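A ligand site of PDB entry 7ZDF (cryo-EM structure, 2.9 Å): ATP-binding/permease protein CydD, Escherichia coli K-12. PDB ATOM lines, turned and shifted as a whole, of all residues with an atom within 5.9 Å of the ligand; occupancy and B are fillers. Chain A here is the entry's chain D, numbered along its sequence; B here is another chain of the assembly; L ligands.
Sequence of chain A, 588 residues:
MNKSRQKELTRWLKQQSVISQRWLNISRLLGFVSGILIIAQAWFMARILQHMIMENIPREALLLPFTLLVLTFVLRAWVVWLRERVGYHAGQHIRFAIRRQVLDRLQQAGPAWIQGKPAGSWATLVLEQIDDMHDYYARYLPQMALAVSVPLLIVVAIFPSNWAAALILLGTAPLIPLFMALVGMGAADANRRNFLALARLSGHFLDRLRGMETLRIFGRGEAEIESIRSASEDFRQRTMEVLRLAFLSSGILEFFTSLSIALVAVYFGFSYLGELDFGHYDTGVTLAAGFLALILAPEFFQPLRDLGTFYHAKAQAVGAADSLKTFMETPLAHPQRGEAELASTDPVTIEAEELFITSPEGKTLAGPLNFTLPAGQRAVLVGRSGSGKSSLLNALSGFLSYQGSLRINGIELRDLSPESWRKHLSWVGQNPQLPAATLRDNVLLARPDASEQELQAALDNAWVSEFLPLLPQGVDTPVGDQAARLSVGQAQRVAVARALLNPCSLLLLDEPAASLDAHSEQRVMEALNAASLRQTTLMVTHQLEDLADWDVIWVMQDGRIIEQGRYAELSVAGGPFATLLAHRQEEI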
ATOM      1  N   ALA A 190      -3.537  16.896  -4.491  1.00  0.00           N
ATOM      2  CA  ALA A 190      -3.700  15.462  -4.750  1.00  0.00           C
ATOM      3  C   ALA A 190      -2.512  14.911  -5.521  1.00  0.00           C
ATOM      4  O   ALA A 190      -2.070  13.785  -5.265  1.00  0.00           O
ATOM      5  CB  ALA A 190      -4.995  15.221  -5.523  1.00  0.00           C
ATOM      6  N   ASN A 191      -1.986  15.684  -6.472  1.00  0.00           N
ATOM      7  CA  ASN A 191      -0.778  15.285  -7.173  1.00  0.00           C
ATOM      8  C   ASN A 191       0.407  15.209  -6.216  1.00  0.00           C
ATOM      9  O   ASN A 191       1.230  14.290  -6.305  1.00  0.00           O
ATOM     10  CB  ASN A 191      -0.473  16.255  -8.310  1.00  0.00           C
ATOM     11  CG  ASN A 191      -1.092  15.818  -9.623  1.00  0.00           C
ATOM     12  OD1 ASN A 191      -1.672  14.735  -9.723  1.00  0.00           O
ATOM     13  ND2 ASN A 191      -0.980  16.664 -10.631  1.00  0.00           N
ATOM     14  N   ARG A 192       0.508  16.175  -5.298  1.00  0.00           N
ATOM     15  CA  ARG A 192       1.605  16.147  -4.322  1.00  0.00           C
ATOM     16  C   ARG A 192       1.528  14.904  -3.450  1.00  0.00           C
ATOM     17  O   ARG A 192       2.561  14.332  -3.093  1.00  0.00           O
ATOM     18  CB  ARG A 192       1.559  17.410  -3.465  1.00  0.00           C
ATOM     19  CG  ARG A 192       2.622  17.441  -2.386  1.00  0.00           C
ATOM     20  CD  ARG A 192       2.252  18.415  -1.274  1.00  0.00           C
ATOM     21  NE  ARG A 192       1.029  18.019  -0.597  1.00  0.00           N
ATOM     22  CZ  ARG A 192       1.004  17.358   0.551  1.00  0.00           C
ATOM     23  NH1 ARG A 192      -0.154  17.039   1.110  1.00  0.00           N
ATOM     24  NH2 ARG A 192       2.136  17.008   1.147  1.00  0.00           N
ATOM     25  N   ASN A 194       0.221  12.085  -4.489  1.00  0.00           N
ATOM     26  CA  ASN A 194       0.583  10.987  -5.379  1.00  0.00           C
ATOM     27  C   ASN A 194       2.085  10.794  -5.470  1.00  0.00           C
ATOM     28  O   ASN A 194       2.556   9.666  -5.583  1.00  0.00           O
ATOM     29  CB  ASN A 194      -0.003  11.210  -6.766  1.00  0.00           C
ATOM     30  CG  ASN A 194      -1.500  11.028  -6.812  1.00  0.00           C
ATOM     31  OD1 ASN A 194      -2.179  11.584  -7.655  1.00  0.00           O
ATOM     32  ND2 ASN A 194      -2.016  10.216  -5.896  1.00  0.00           N
ATOM     33  N   PHE A 195       2.847  11.885  -5.430  1.00  0.00           N
ATOM     34  CA  PHE A 195       4.303  11.762  -5.425  1.00  0.00           C
ATOM     35  C   PHE A 195       4.794  11.158  -4.114  1.00  0.00           C
ATOM     36  O   PHE A 195       5.760  10.384  -4.111  1.00  0.00           O
ATOM     37  CB  PHE A 195       4.952  13.127  -5.661  1.00  0.00           C
ATOM     38  CG  PHE A 195       4.906  13.583  -7.080  1.00  0.00           C
ATOM     39  CD1 PHE A 195       5.718  13.007  -8.035  1.00  0.00           C
ATOM     40  CD2 PHE A 195       4.052  14.604  -7.466  1.00  0.00           C
ATOM     41  CE1 PHE A 195       5.678  13.421  -9.349  1.00  0.00           C
ATOM     42  CE2 PHE A 195       4.007  15.024  -8.775  1.00  0.00           C
ATOM     43  CZ  PHE A 195       4.827  14.430  -9.717  1.00  0.00           C
ATOM     44  N   LEU A 198       4.191   7.531  -4.537  1.00  0.00           N
ATOM     45  CA  LEU A 198       5.209   6.931  -5.402  1.00  0.00           C
ATOM     46  C   LEU A 198       6.523   6.734  -4.664  1.00  0.00           C
ATOM     47  O   LEU A 198       7.194   5.713  -4.833  1.00  0.00           O
ATOM     48  CB  LEU A 198       5.412   7.791  -6.654  1.00  0.00           C
ATOM     49  CG  LEU A 198       6.484   7.303  -7.635  1.00  0.00           C
ATOM     50  CD1 LEU A 198       6.059   6.023  -8.324  1.00  0.00           C
ATOM     51  CD2 LEU A 198       6.802   8.387  -8.655  1.00  0.00           C
ATOM     52  N   PHE A 235      -1.301   1.718  -6.728  1.00  0.00           N
ATOM     53  CA  PHE A 235      -0.775   3.073  -6.900  1.00  0.00           C
ATOM     54  C   PHE A 235      -1.165   3.640  -8.255  1.00  0.00           C
ATOM     55  O   PHE A 235      -1.600   4.798  -8.347  1.00  0.00           O
ATOM     56  CB  PHE A 235       0.751   3.080  -6.741  1.00  0.00           C
ATOM     57  CG  PHE A 235       1.409   4.269  -7.366  1.00  0.00           C
ATOM     58  CD1 PHE A 235       1.443   5.490  -6.710  1.00  0.00           C
ATOM     59  CD2 PHE A 235       1.986   4.185  -8.625  1.00  0.00           C
ATOM     60  CE1 PHE A 235       2.039   6.585  -7.290  1.00  0.00           C
ATOM     61  CE2 PHE A 235       2.582   5.280  -9.205  1.00  0.00           C
ATOM     62  CZ  PHE A 235       2.603   6.485  -8.541  1.00  0.00           C
ATOM     63  N   THR A 239      -3.404   6.857  -8.904  1.00  0.00           N
ATOM     64  CA  THR A 239      -2.762   8.023  -9.513  1.00  0.00           C
ATOM     65  C   THR A 239      -3.451   8.411 -10.816  1.00  0.00           C
ATOM     66  O   THR A 239      -3.640   9.601 -11.094  1.00  0.00           O
ATOM     67  CB  THR A 239      -1.282   7.731  -9.753  1.00  0.00           C
ATOM     68  OG1 THR A 239      -0.671   7.376  -8.516  1.00  0.00           O
ATOM     69  CG2 THR A 239      -0.591   8.958 -10.314  1.00  0.00           C
ATOM     70  N   LEU A 243      -4.831  11.935 -12.123  1.00  0.00           N
ATOM     71  CA  LEU A 243      -4.257  12.499 -13.337  1.00  0.00           C
ATOM     72  C   LEU A 243      -5.293  12.750 -14.417  1.00  0.00           C
ATOM     73  O   LEU A 243      -5.033  13.552 -15.330  1.00  0.00           O
ATOM     74  CB  LEU A 243      -3.157  11.582 -13.878  1.00  0.00           C
ATOM     75  CG  LEU A 243      -1.832  11.645 -13.126  1.00  0.00           C
ATOM     76  CD1 LEU A 243      -0.789  10.772 -13.788  1.00  0.00           C
ATOM     77  CD2 LEU A 243      -1.366  13.080 -13.051  1.00  0.00           C
ATOM     78  N   ALA A 246      -5.827  16.322 -13.574  1.00  0.00           N
ATOM     79  CA  ALA A 246      -4.658  17.171 -13.633  1.00  0.00           C
ATOM     80  C   ALA A 246      -4.140  17.374 -15.049  1.00  0.00           C
ATOM     81  O   ALA A 246      -3.445  18.359 -15.312  1.00  0.00           O
ATOM     82  CB  ALA A 246      -3.540  16.595 -12.758  1.00  0.00           C
ATOM     83  N   PHE A 247      -4.466  16.470 -15.970  1.00  0.00           N
ATOM     84  CA  PHE A 247      -4.067  16.608 -17.362  1.00  0.00           C
ATOM     85  C   PHE A 247      -5.060  17.409 -18.173  1.00  0.00           C
ATOM     86  O   PHE A 247      -4.808  17.676 -19.358  1.00  0.00           O
ATOM     87  CB  PHE A 247      -3.879  15.223 -18.000  1.00  0.00           C
ATOM     88  CG  PHE A 247      -2.615  14.540 -17.587  1.00  0.00           C
ATOM     89  CD1 PHE A 247      -1.464  15.267 -17.353  1.00  0.00           C
ATOM     90  CD2 PHE A 247      -2.572  13.170 -17.436  1.00  0.00           C
ATOM     91  CE1 PHE A 247      -0.296  14.653 -16.977  1.00  0.00           C
ATOM     92  CE2 PHE A 247      -1.401  12.543 -17.058  1.00  0.00           C
ATOM     93  CZ  PHE A 247      -0.265  13.288 -16.826  1.00  0.00           C
ATOM     94  N   SER A 249      -5.719  20.545 -17.543  1.00  0.00           N
ATOM     95  CA  SER A 249      -5.066  21.836 -17.691  1.00  0.00           C
ATOM     96  C   SER A 249      -4.116  21.846 -18.888  1.00  0.00           C
ATOM     97  O   SER A 249      -4.046  22.830 -19.629  1.00  0.00           O
ATOM     98  CB  SER A 249      -4.320  22.207 -16.413  1.00  0.00           C
ATOM     99  OG  SER A 249      -5.108  21.939 -15.271  1.00  0.00           O
ATOM    100  N   SER A 250      -3.364  20.753 -19.072  1.00  0.00           N
ATOM    101  CA  SER A 250      -2.520  20.628 -20.252  1.00  0.00           C
ATOM    102  C   SER A 250      -3.350  20.611 -21.526  1.00  0.00           C
ATOM    103  O   SER A 250      -2.984  21.234 -22.521  1.00  0.00           O
ATOM    104  CB  SER A 250      -1.663  19.372 -20.140  1.00  0.00           C
ATOM    105  OG  SER A 250      -0.943  19.137 -21.341  1.00  0.00           O
ATOM    106  N   LEU A 307       5.612  26.041 -19.253  1.00  0.00           N
ATOM    107  CA  LEU A 307       5.489  25.932 -17.809  1.00  0.00           C
ATOM    108  C   LEU A 307       4.954  24.563 -17.407  1.00  0.00           C
ATOM    109  O   LEU A 307       5.208  24.111 -16.275  1.00  0.00           O
ATOM    110  CB  LEU A 307       4.571  27.039 -17.278  1.00  0.00           C
ATOM    111  CG  LEU A 307       4.627  27.339 -15.788  1.00  0.00           C
ATOM    112  CD1 LEU A 307       6.035  27.660 -15.345  1.00  0.00           C
ATOM    113  CD2 LEU A 307       3.689  28.486 -15.455  1.00  0.00           C
ATOM    114  N   GLY A 308       4.220  23.891 -18.298  1.00  0.00           N
ATOM    115  CA  GLY A 308       3.815  22.525 -18.022  1.00  0.00           C
ATOM    116  C   GLY A 308       4.929  21.534 -18.226  1.00  0.00           C
ATOM    117  O   GLY A 308       4.938  20.470 -17.610  1.00  0.00           O
ATOM    118  N   THR A 309       5.889  21.863 -19.090  1.00  0.00           N
ATOM    119  CA  THR A 309       7.081  21.044 -19.227  1.00  0.00           C
ATOM    120  C   THR A 309       7.869  21.026 -17.929  1.00  0.00           C
ATOM    121  O   THR A 309       8.420  19.986 -17.536  1.00  0.00           O
ATOM    122  CB  THR A 309       7.941  21.552 -20.383  1.00  0.00           C
ATOM    123  OG1 THR A 309       7.310  21.217 -21.629  1.00  0.00           O
ATOM    124  CG2 THR A 309       9.336  20.953 -20.348  1.00  0.00           C
ATOM    125  N   PHE A 310       7.927  22.164 -17.232  1.00  0.00           N
ATOM    126  CA  PHE A 310       8.656  22.301 -15.989  1.00  0.00           C
ATOM    127  C   PHE A 310       7.826  21.888 -14.773  1.00  0.00           C
ATOM    128  O   PHE A 310       8.142  22.322 -13.654  1.00  0.00           O
ATOM    129  CB  PHE A 310       9.130  23.745 -15.817  1.00  0.00           C
ATOM    130  CG  PHE A 310      10.055  24.204 -16.897  1.00  0.00           C
ATOM    131  CD1 PHE A 310      10.914  23.320 -17.517  1.00  0.00           C
ATOM    132  CD2 PHE A 310      10.060  25.528 -17.294  1.00  0.00           C
ATOM    133  CE1 PHE A 310      11.769  23.754 -18.516  1.00  0.00           C
ATOM    134  CE2 PHE A 310      10.915  25.962 -18.293  1.00  0.00           C
ATOM    135  CZ  PHE A 310      11.765  25.072 -18.895  1.00  0.00           C
ATOM    136  N   TYR A 311       6.778  21.094 -14.965  1.00  0.00           N
ATOM    137  CA  TYR A 311       5.929  20.708 -13.845  1.00  0.00           C
ATOM    138  C   TYR A 311       6.702  19.907 -12.805  1.00  0.00           C
ATOM    139  O   TYR A 311       6.545  20.130 -11.595  1.00  0.00           O
ATOM    140  CB  TYR A 311       4.738  19.892 -14.339  1.00  0.00           C
ATOM    141  CG  TYR A 311       3.972  19.215 -13.231  1.00  0.00           C
ATOM    142  CD1 TYR A 311       3.027  19.915 -12.489  1.00  0.00           C
ATOM    143  CD2 TYR A 311       4.204  17.886 -12.916  1.00  0.00           C
ATOM    144  CE1 TYR A 311       2.335  19.300 -11.468  1.00  0.00           C
ATOM    145  CE2 TYR A 311       3.504  17.268 -11.901  1.00  0.00           C
ATOM    146  CZ  TYR A 311       2.570  17.975 -11.177  1.00  0.00           C
ATOM    147  OH  TYR A 311       1.880  17.366 -10.163  1.00  0.00           O
ATOM    148  N   HIS A 312       7.546  18.986 -13.250  1.00  0.00           N
ATOM    149  CA  HIS A 312       8.256  18.121 -12.310  1.00  0.00           C
ATOM    150  C   HIS A 312       9.325  18.876 -11.541  1.00  0.00           C
ATOM    151  O   HIS A 312       9.695  18.459 -10.434  1.00  0.00           O
ATOM    152  CB  HIS A 312       8.863  16.943 -13.049  1.00  0.00           C
ATOM    153  CG  HIS A 312       7.935  15.793 -13.205  1.00  0.00           C
ATOM    154  ND1 HIS A 312       7.319  15.185 -12.135  1.00  0.00           N
ATOM    155  CD2 HIS A 312       7.488  15.144 -14.305  1.00  0.00           C
ATOM    156  CE1 HIS A 312       6.541  14.204 -12.565  1.00  0.00           C
ATOM    157  NE2 HIS A 312       6.627  14.162 -13.880  1.00  0.00           N
ATOM    158  N   ARG B  77      -3.197  15.782 -26.991  1.00  0.00           N
ATOM    159  CA  ARG B  77      -2.298  16.130 -25.901  1.00  0.00           C
ATOM    160  C   ARG B  77      -2.802  15.559 -24.583  1.00  0.00           C
ATOM    161  O   ARG B  77      -2.012  15.066 -23.770  1.00  0.00           O
ATOM    162  CB  ARG B  77      -2.148  17.647 -25.811  1.00  0.00           C
ATOM    163  CG  ARG B  77      -1.531  18.169 -24.516  1.00  0.00           C
ATOM    164  CD  ARG B  77      -0.161  17.575 -24.253  1.00  0.00           C
ATOM    165  NE  ARG B  77       0.741  17.737 -25.389  1.00  0.00           N
ATOM    166  CZ  ARG B  77       1.524  18.788 -25.571  1.00  0.00           C
ATOM    167  NH1 ARG B  77       2.319  18.858 -26.632  1.00  0.00           N
ATOM    168  NH2 ARG B  77       1.516  19.784 -24.689  1.00  0.00           N
ATOM    169  N   ARG B  81      -0.625  12.430 -22.638  1.00  0.00           N
ATOM    170  CA  ARG B  81      -0.201  12.488 -21.246  1.00  0.00           C
ATOM    171  C   ARG B  81      -0.794  11.345 -20.438  1.00  0.00           C
ATOM    172  O   ARG B  81      -0.113  10.752 -19.601  1.00  0.00           O
ATOM    173  CB  ARG B  81      -0.579  13.835 -20.638  1.00  0.00           C
ATOM    174  CG  ARG B  81       0.130  15.020 -21.263  1.00  0.00           C
ATOM    175  CD  ARG B  81       1.487  15.239 -20.634  1.00  0.00           C
ATOM    176  NE  ARG B  81       2.084  16.503 -21.046  1.00  0.00           N
ATOM    177  CZ  ARG B  81       2.868  16.651 -22.106  1.00  0.00           C
ATOM    178  NH1 ARG B  81       3.370  17.837 -22.410  1.00  0.00           N
ATOM    179  NH2 ARG B  81       3.174  15.597 -22.855  1.00  0.00           N
ATOM    180  N   HIS B  85       1.534   7.975 -19.303  1.00  0.00           N
ATOM    181  CA  HIS B  85       1.750   7.922 -17.860  1.00  0.00           C
ATOM    182  C   HIS B  85       1.247   6.616 -17.270  1.00  0.00           C
ATOM    183  O   HIS B  85       1.877   6.073 -16.357  1.00  0.00           O
ATOM    184  CB  HIS B  85       1.052   9.095 -17.187  1.00  0.00           C
ATOM    185  CG  HIS B  85       1.856  10.356 -17.196  1.00  0.00           C
ATOM    186  ND1 HIS B  85       2.153  11.030 -18.354  1.00  0.00           N
ATOM    187  CD2 HIS B  85       2.439  11.049 -16.194  1.00  0.00           C
ATOM    188  CE1 HIS B  85       2.886  12.092 -18.063  1.00  0.00           C
ATOM    189  NE2 HIS B  85       3.067  12.130 -16.760  1.00  0.00           N
ATOM    190  N   THR B  88       3.914   4.233 -18.343  1.00  0.00           N
ATOM    191  CA  THR B  88       5.114   4.352 -17.520  1.00  0.00           C
ATOM    192  C   THR B  88       4.970   3.585 -16.213  1.00  0.00           C
ATOM    193  O   THR B  88       5.925   2.938 -15.756  1.00  0.00           O
ATOM    194  CB  THR B  88       5.412   5.832 -17.242  1.00  0.00           C
ATOM    195  OG1 THR B  88       5.711   6.486 -18.490  1.00  0.00           O
ATOM    196  CG2 THR B  88       6.599   5.984 -16.319  1.00  0.00           C
ATOM    197  N   PHE B  89       3.799   3.637 -15.597  1.00  0.00           N
ATOM    198  CA  PHE B  89       3.569   2.877 -14.371  1.00  0.00           C
ATOM    199  C   PHE B  89       3.417   1.386 -14.639  1.00  0.00           C
ATOM    200  O   PHE B  89       3.625   0.579 -13.728  1.00  0.00           O
ATOM    201  CB  PHE B  89       2.346   3.409 -13.630  1.00  0.00           C
ATOM    202  CG  PHE B  89       2.403   4.884 -13.339  1.00  0.00           C
ATOM    203  CD1 PHE B  89       3.608   5.504 -13.062  1.00  0.00           C
ATOM    204  CD2 PHE B  89       1.251   5.635 -13.327  1.00  0.00           C
ATOM    205  CE1 PHE B  89       3.655   6.857 -12.793  1.00  0.00           C
ATOM    206  CE2 PHE B  89       1.285   6.992 -13.059  1.00  0.00           C
ATOM    207  CZ  PHE B  89       2.500   7.599 -12.792  1.00  0.00           C
ATOM    208  N   ASP B 128      14.187   2.846 -11.192  1.00  0.00           N
ATOM    209  CA  ASP B 128      13.474   4.071 -11.531  1.00  0.00           C
ATOM    210  C   ASP B 128      14.024   4.693 -12.811  1.00  0.00           C
ATOM    211  O   ASP B 128      13.274   5.191 -13.649  1.00  0.00           O
ATOM    212  CB  ASP B 128      13.563   5.060 -10.376  1.00  0.00           C
ATOM    213  CG  ASP B 128      12.496   4.821  -9.329  1.00  0.00           C
ATOM    214  OD1 ASP B 128      11.298   4.850  -9.672  1.00  0.00           O
ATOM    215  OD2 ASP B 128      12.861   4.596  -8.151  1.00  0.00           O
ATOM    216  N   ASP B 131      12.908   3.081 -15.835  1.00  0.00           N
ATOM    217  CA  ASP B 131      11.521   3.446 -16.099  1.00  0.00           C
ATOM    218  C   ASP B 131      11.406   4.741 -16.885  1.00  0.00           C
ATOM    219  O   ASP B 131      10.368   4.991 -17.504  1.00  0.00           O
ATOM    220  CB  ASP B 131      10.762   3.544 -14.772  1.00  0.00           C
ATOM    221  CG  ASP B 131       9.290   3.836 -14.964  1.00  0.00           C
ATOM    222  OD1 ASP B 131       8.743   4.657 -14.209  1.00  0.00           O
ATOM    223  OD2 ASP B 131       8.678   3.238 -15.868  1.00  0.00           O
ATOM    224  N   HIS B 132      12.450   5.558 -16.889  1.00  0.00           N
ATOM    225  CA  HIS B 132      12.469   6.835 -17.589  1.00  0.00           C
ATOM    226  C   HIS B 132      12.845   6.694 -19.062  1.00  0.00           C
ATOM    227  O   HIS B 132      12.876   7.696 -19.769  1.00  0.00           O
ATOM    228  CB  HIS B 132      13.439   7.804 -16.918  1.00  0.00           C
ATOM    229  CG  HIS B 132      13.122   8.076 -15.483  1.00  0.00           C
ATOM    230  ND1 HIS B 132      14.005   8.701 -14.631  1.00  0.00           N
ATOM    231  CD2 HIS B 132      12.005   7.826 -14.755  1.00  0.00           C
ATOM    232  CE1 HIS B 132      13.452   8.809 -13.440  1.00  0.00           C
ATOM    233  NE2 HIS B 132      12.240   8.293 -13.487  1.00  0.00           N
ATOM    234  N   LEU B 135       9.372   7.627 -21.571  1.00  0.00           N
ATOM    235  CA  LEU B 135       8.923   9.011 -21.690  1.00  0.00           C
ATOM    236  C   LEU B 135      10.069   9.987 -21.906  1.00  0.00           C
ATOM    237  O   LEU B 135       9.900  10.992 -22.608  1.00  0.00           O
ATOM    238  CB  LEU B 135       8.122   9.429 -20.466  1.00  0.00           C
ATOM    239  CG  LEU B 135       6.630   9.169 -20.560  1.00  0.00           C
ATOM    240  CD1 LEU B 135       5.929   9.600 -19.289  1.00  0.00           C
ATOM    241  CD2 LEU B 135       6.103   9.943 -21.743  1.00  0.00           C
ATOM    242  N   ARG B 136      11.229   9.746 -21.310  1.00  0.00           N
ATOM    243  CA  ARG B 136      12.292  10.730 -21.344  1.00  0.00           C
ATOM    244  C   ARG B 136      13.329  10.467 -22.434  1.00  0.00           C
ATOM    245  O   ARG B 136      14.159  11.343 -22.685  1.00  0.00           O
ATOM    246  CB  ARG B 136      12.983  10.824 -19.983  1.00  0.00           C
ATOM    247  CG  ARG B 136      12.063  11.304 -18.870  1.00  0.00           C
ATOM    248  CD  ARG B 136      12.836  11.972 -17.753  1.00  0.00           C
ATOM    249  NE  ARG B 136      12.010  12.156 -16.553  1.00  0.00           N
ATOM    250  CZ  ARG B 136      11.165  13.170 -16.378  1.00  0.00           C
ATOM    251  NH1 ARG B 136      11.028  14.098 -17.303  1.00  0.00           N
ATOM    252  NH2 ARG B 136      10.461  13.243 -15.259  1.00  0.00           N
HETATM  253 FE1  LIG L   1       4.725  13.028 -15.066  1.00  0.00          FE
HETATM  254  N1  LIG L   1       5.571  13.772 -16.863  1.00  0.00           N
HETATM  255  N2  LIG L   1       6.144  11.397 -14.987  1.00  0.00           N
HETATM  256  N3  LIG L   1       3.761  12.403 -13.237  1.00  0.00           N
HETATM  257  N4  LIG L   1       3.138  14.764 -15.028  1.00  0.00           N
HETATM  258  C1  LIG L   1       5.160  14.943 -17.628  1.00  0.00           C
HETATM  259  O1  LIG L   1       7.768  17.472 -21.511  1.00  0.00           O
HETATM  260  C2  LIG L   1       7.204  11.125 -15.976  1.00  0.00           C
HETATM  261  C3  LIG L   1       4.200  11.182 -12.453  1.00  0.00           C
HETATM  262  C4  LIG L   1       2.132  14.934 -14.019  1.00  0.00           C
HETATM  263  O2  LIG L   1       1.777  19.216 -19.279  1.00  0.00           O
HETATM  264  C5  LIG L   1       6.043  14.875 -18.607  1.00  0.00           C
HETATM  265  O3  LIG L   1       9.161  17.254 -19.839  1.00  0.00           O
HETATM  266  C6  LIG L   1       7.714  10.061 -15.433  1.00  0.00           C
HETATM  267  C7  LIG L   1       3.413  11.177 -11.513  1.00  0.00           C
HETATM  268  C8  LIG L   1       1.565  16.028 -14.524  1.00  0.00           C
HETATM  269  O4  LIG L   1       0.978  20.557 -17.764  1.00  0.00           O
HETATM  270  C9  LIG L   1       6.891  13.968 -18.646  1.00  0.00           C
HETATM  271  C10 LIG L   1       7.251   9.599 -14.384  1.00  0.00           C
HETATM  272  C11 LIG L   1       2.551  12.045 -11.416  1.00  0.00           C
HETATM  273  C12 LIG L   1       1.991  16.641 -15.682  1.00  0.00           C
HETATM  274  C13 LIG L   1       6.777  13.121 -17.597  1.00  0.00           C
HETATM  275  C14 LIG L   1       6.198  10.339 -13.929  1.00  0.00           C
HETATM  276  C15 LIG L   1       2.628  12.981 -12.506  1.00  0.00           C
HETATM  277  C16 LIG L   1       3.125  15.809 -16.142  1.00  0.00           C
HETATM  278  C17 LIG L   1       6.005  15.938 -19.713  1.00  0.00           C
HETATM  279  C18 LIG L   1       7.789   8.358 -13.687  1.00  0.00           C
HETATM  280  C19 LIG L   1       1.556  12.075 -10.282  1.00  0.00           C
HETATM  281  C20 LIG L   1       1.367  17.896 -16.308  1.00  0.00           C
HETATM  282  C21 LIG L   1       6.806  17.167 -19.320  1.00  0.00           C
HETATM  283  C22 LIG L   1       8.503   8.743 -12.422  1.00  0.00           C
HETATM  284  C23 LIG L   1       1.310  13.438  -9.656  1.00  0.00           C
HETATM  285  C24 LIG L   1       2.390  18.767 -16.990  1.00  0.00           C
HETATM  286  C25 LIG L   1       7.979  17.302 -20.273  1.00  0.00           C
HETATM  287  C26 LIG L   1       1.674  19.559 -18.076  1.00  0.00           C
HETATM  288  C27 LIG L   1       4.070  15.895 -17.367  1.00  0.00           C
HETATM  289  C28 LIG L   1       7.530  11.906 -17.191  1.00  0.00           C
HETATM  290  C29 LIG L   1       5.332  10.219 -12.754  1.00  0.00           C
HETATM  291  C30 LIG L   1       1.877  14.094 -12.809  1.00  0.00           C
HETATM  292  C31 LIG L   1       7.947  13.811 -19.740  1.00  0.00           C
HETATM  293  C32 LIG L   1       8.890   9.389 -16.111  1.00  0.00           C
HETATM  294  C33 LIG L   1       3.498  10.096 -10.453  1.00  0.00           C
HETATM  295  C34 LIG L   1       0.404  16.636 -13.802  1.00  0.00           C
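A ring nitrogen (NE2) of His 312 binds an iron atom (FE1) of the ligand, at 2.5 Å. A ring nitrogen (NE2) of His 85 of chain B is bound to an iron atom (FE1) of the ligand (2.5 Å). The guanidinium group (NE) of Arg 81 of chain B is in salt-bridge range of an oxygen (O2) of the ligand. OG of Ser 250 is in hydrogen-bond range of O2 of the ligand.
The backbone carbonyl oxygen (O) of Arg 81 of chain B is in hydrogen-bond range of a ring nitrogen (ND1) of His 85 of chain B (2.6 Å). The side-chain amide nitrogen (ND2) of Asn 191 sits at hydrogen-bond distance from the side-chain hydroxyl (OH) of Tyr 311 (3.0 Å). NE2 of His 132 of chain B lies close to O of Asp 128 of chain B (3.3 Å). The side-chain hydroxyl (OG1) of Thr 239 sits at hydrogen-bond distance from the backbone carbonyl oxygen (O) of Phe 235, 2.7 Å away. OD1 of Asn 194 sits close to O of Ala 190, 3.3 Å away.
Merely in contact with the ligand: Gly 308, Phe 195, Asn 191, Phe 247, Leu 243, Tyr 311, Leu 135 of chain B, Phe 89 of chain B, Thr 309, Thr 88 of chain B, His 132 of chain B, Arg 136 of chain B, Thr 239, Asp 131 of chain B and Asn 194. Hydrophobic or aromatic side chains that line the ligand: Phe 195, Leu 243, Phe 247, Tyr 311, His 312, His 85 of chain B, Phe 89 of chain B, His 132 of chain B and Leu 135 of chain B. Along chain A the residues within 4 Å of the ligand span positions 191 to 312. The nearest printed residue that does not touch the ligand is Ala 246 (4.1 Å).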
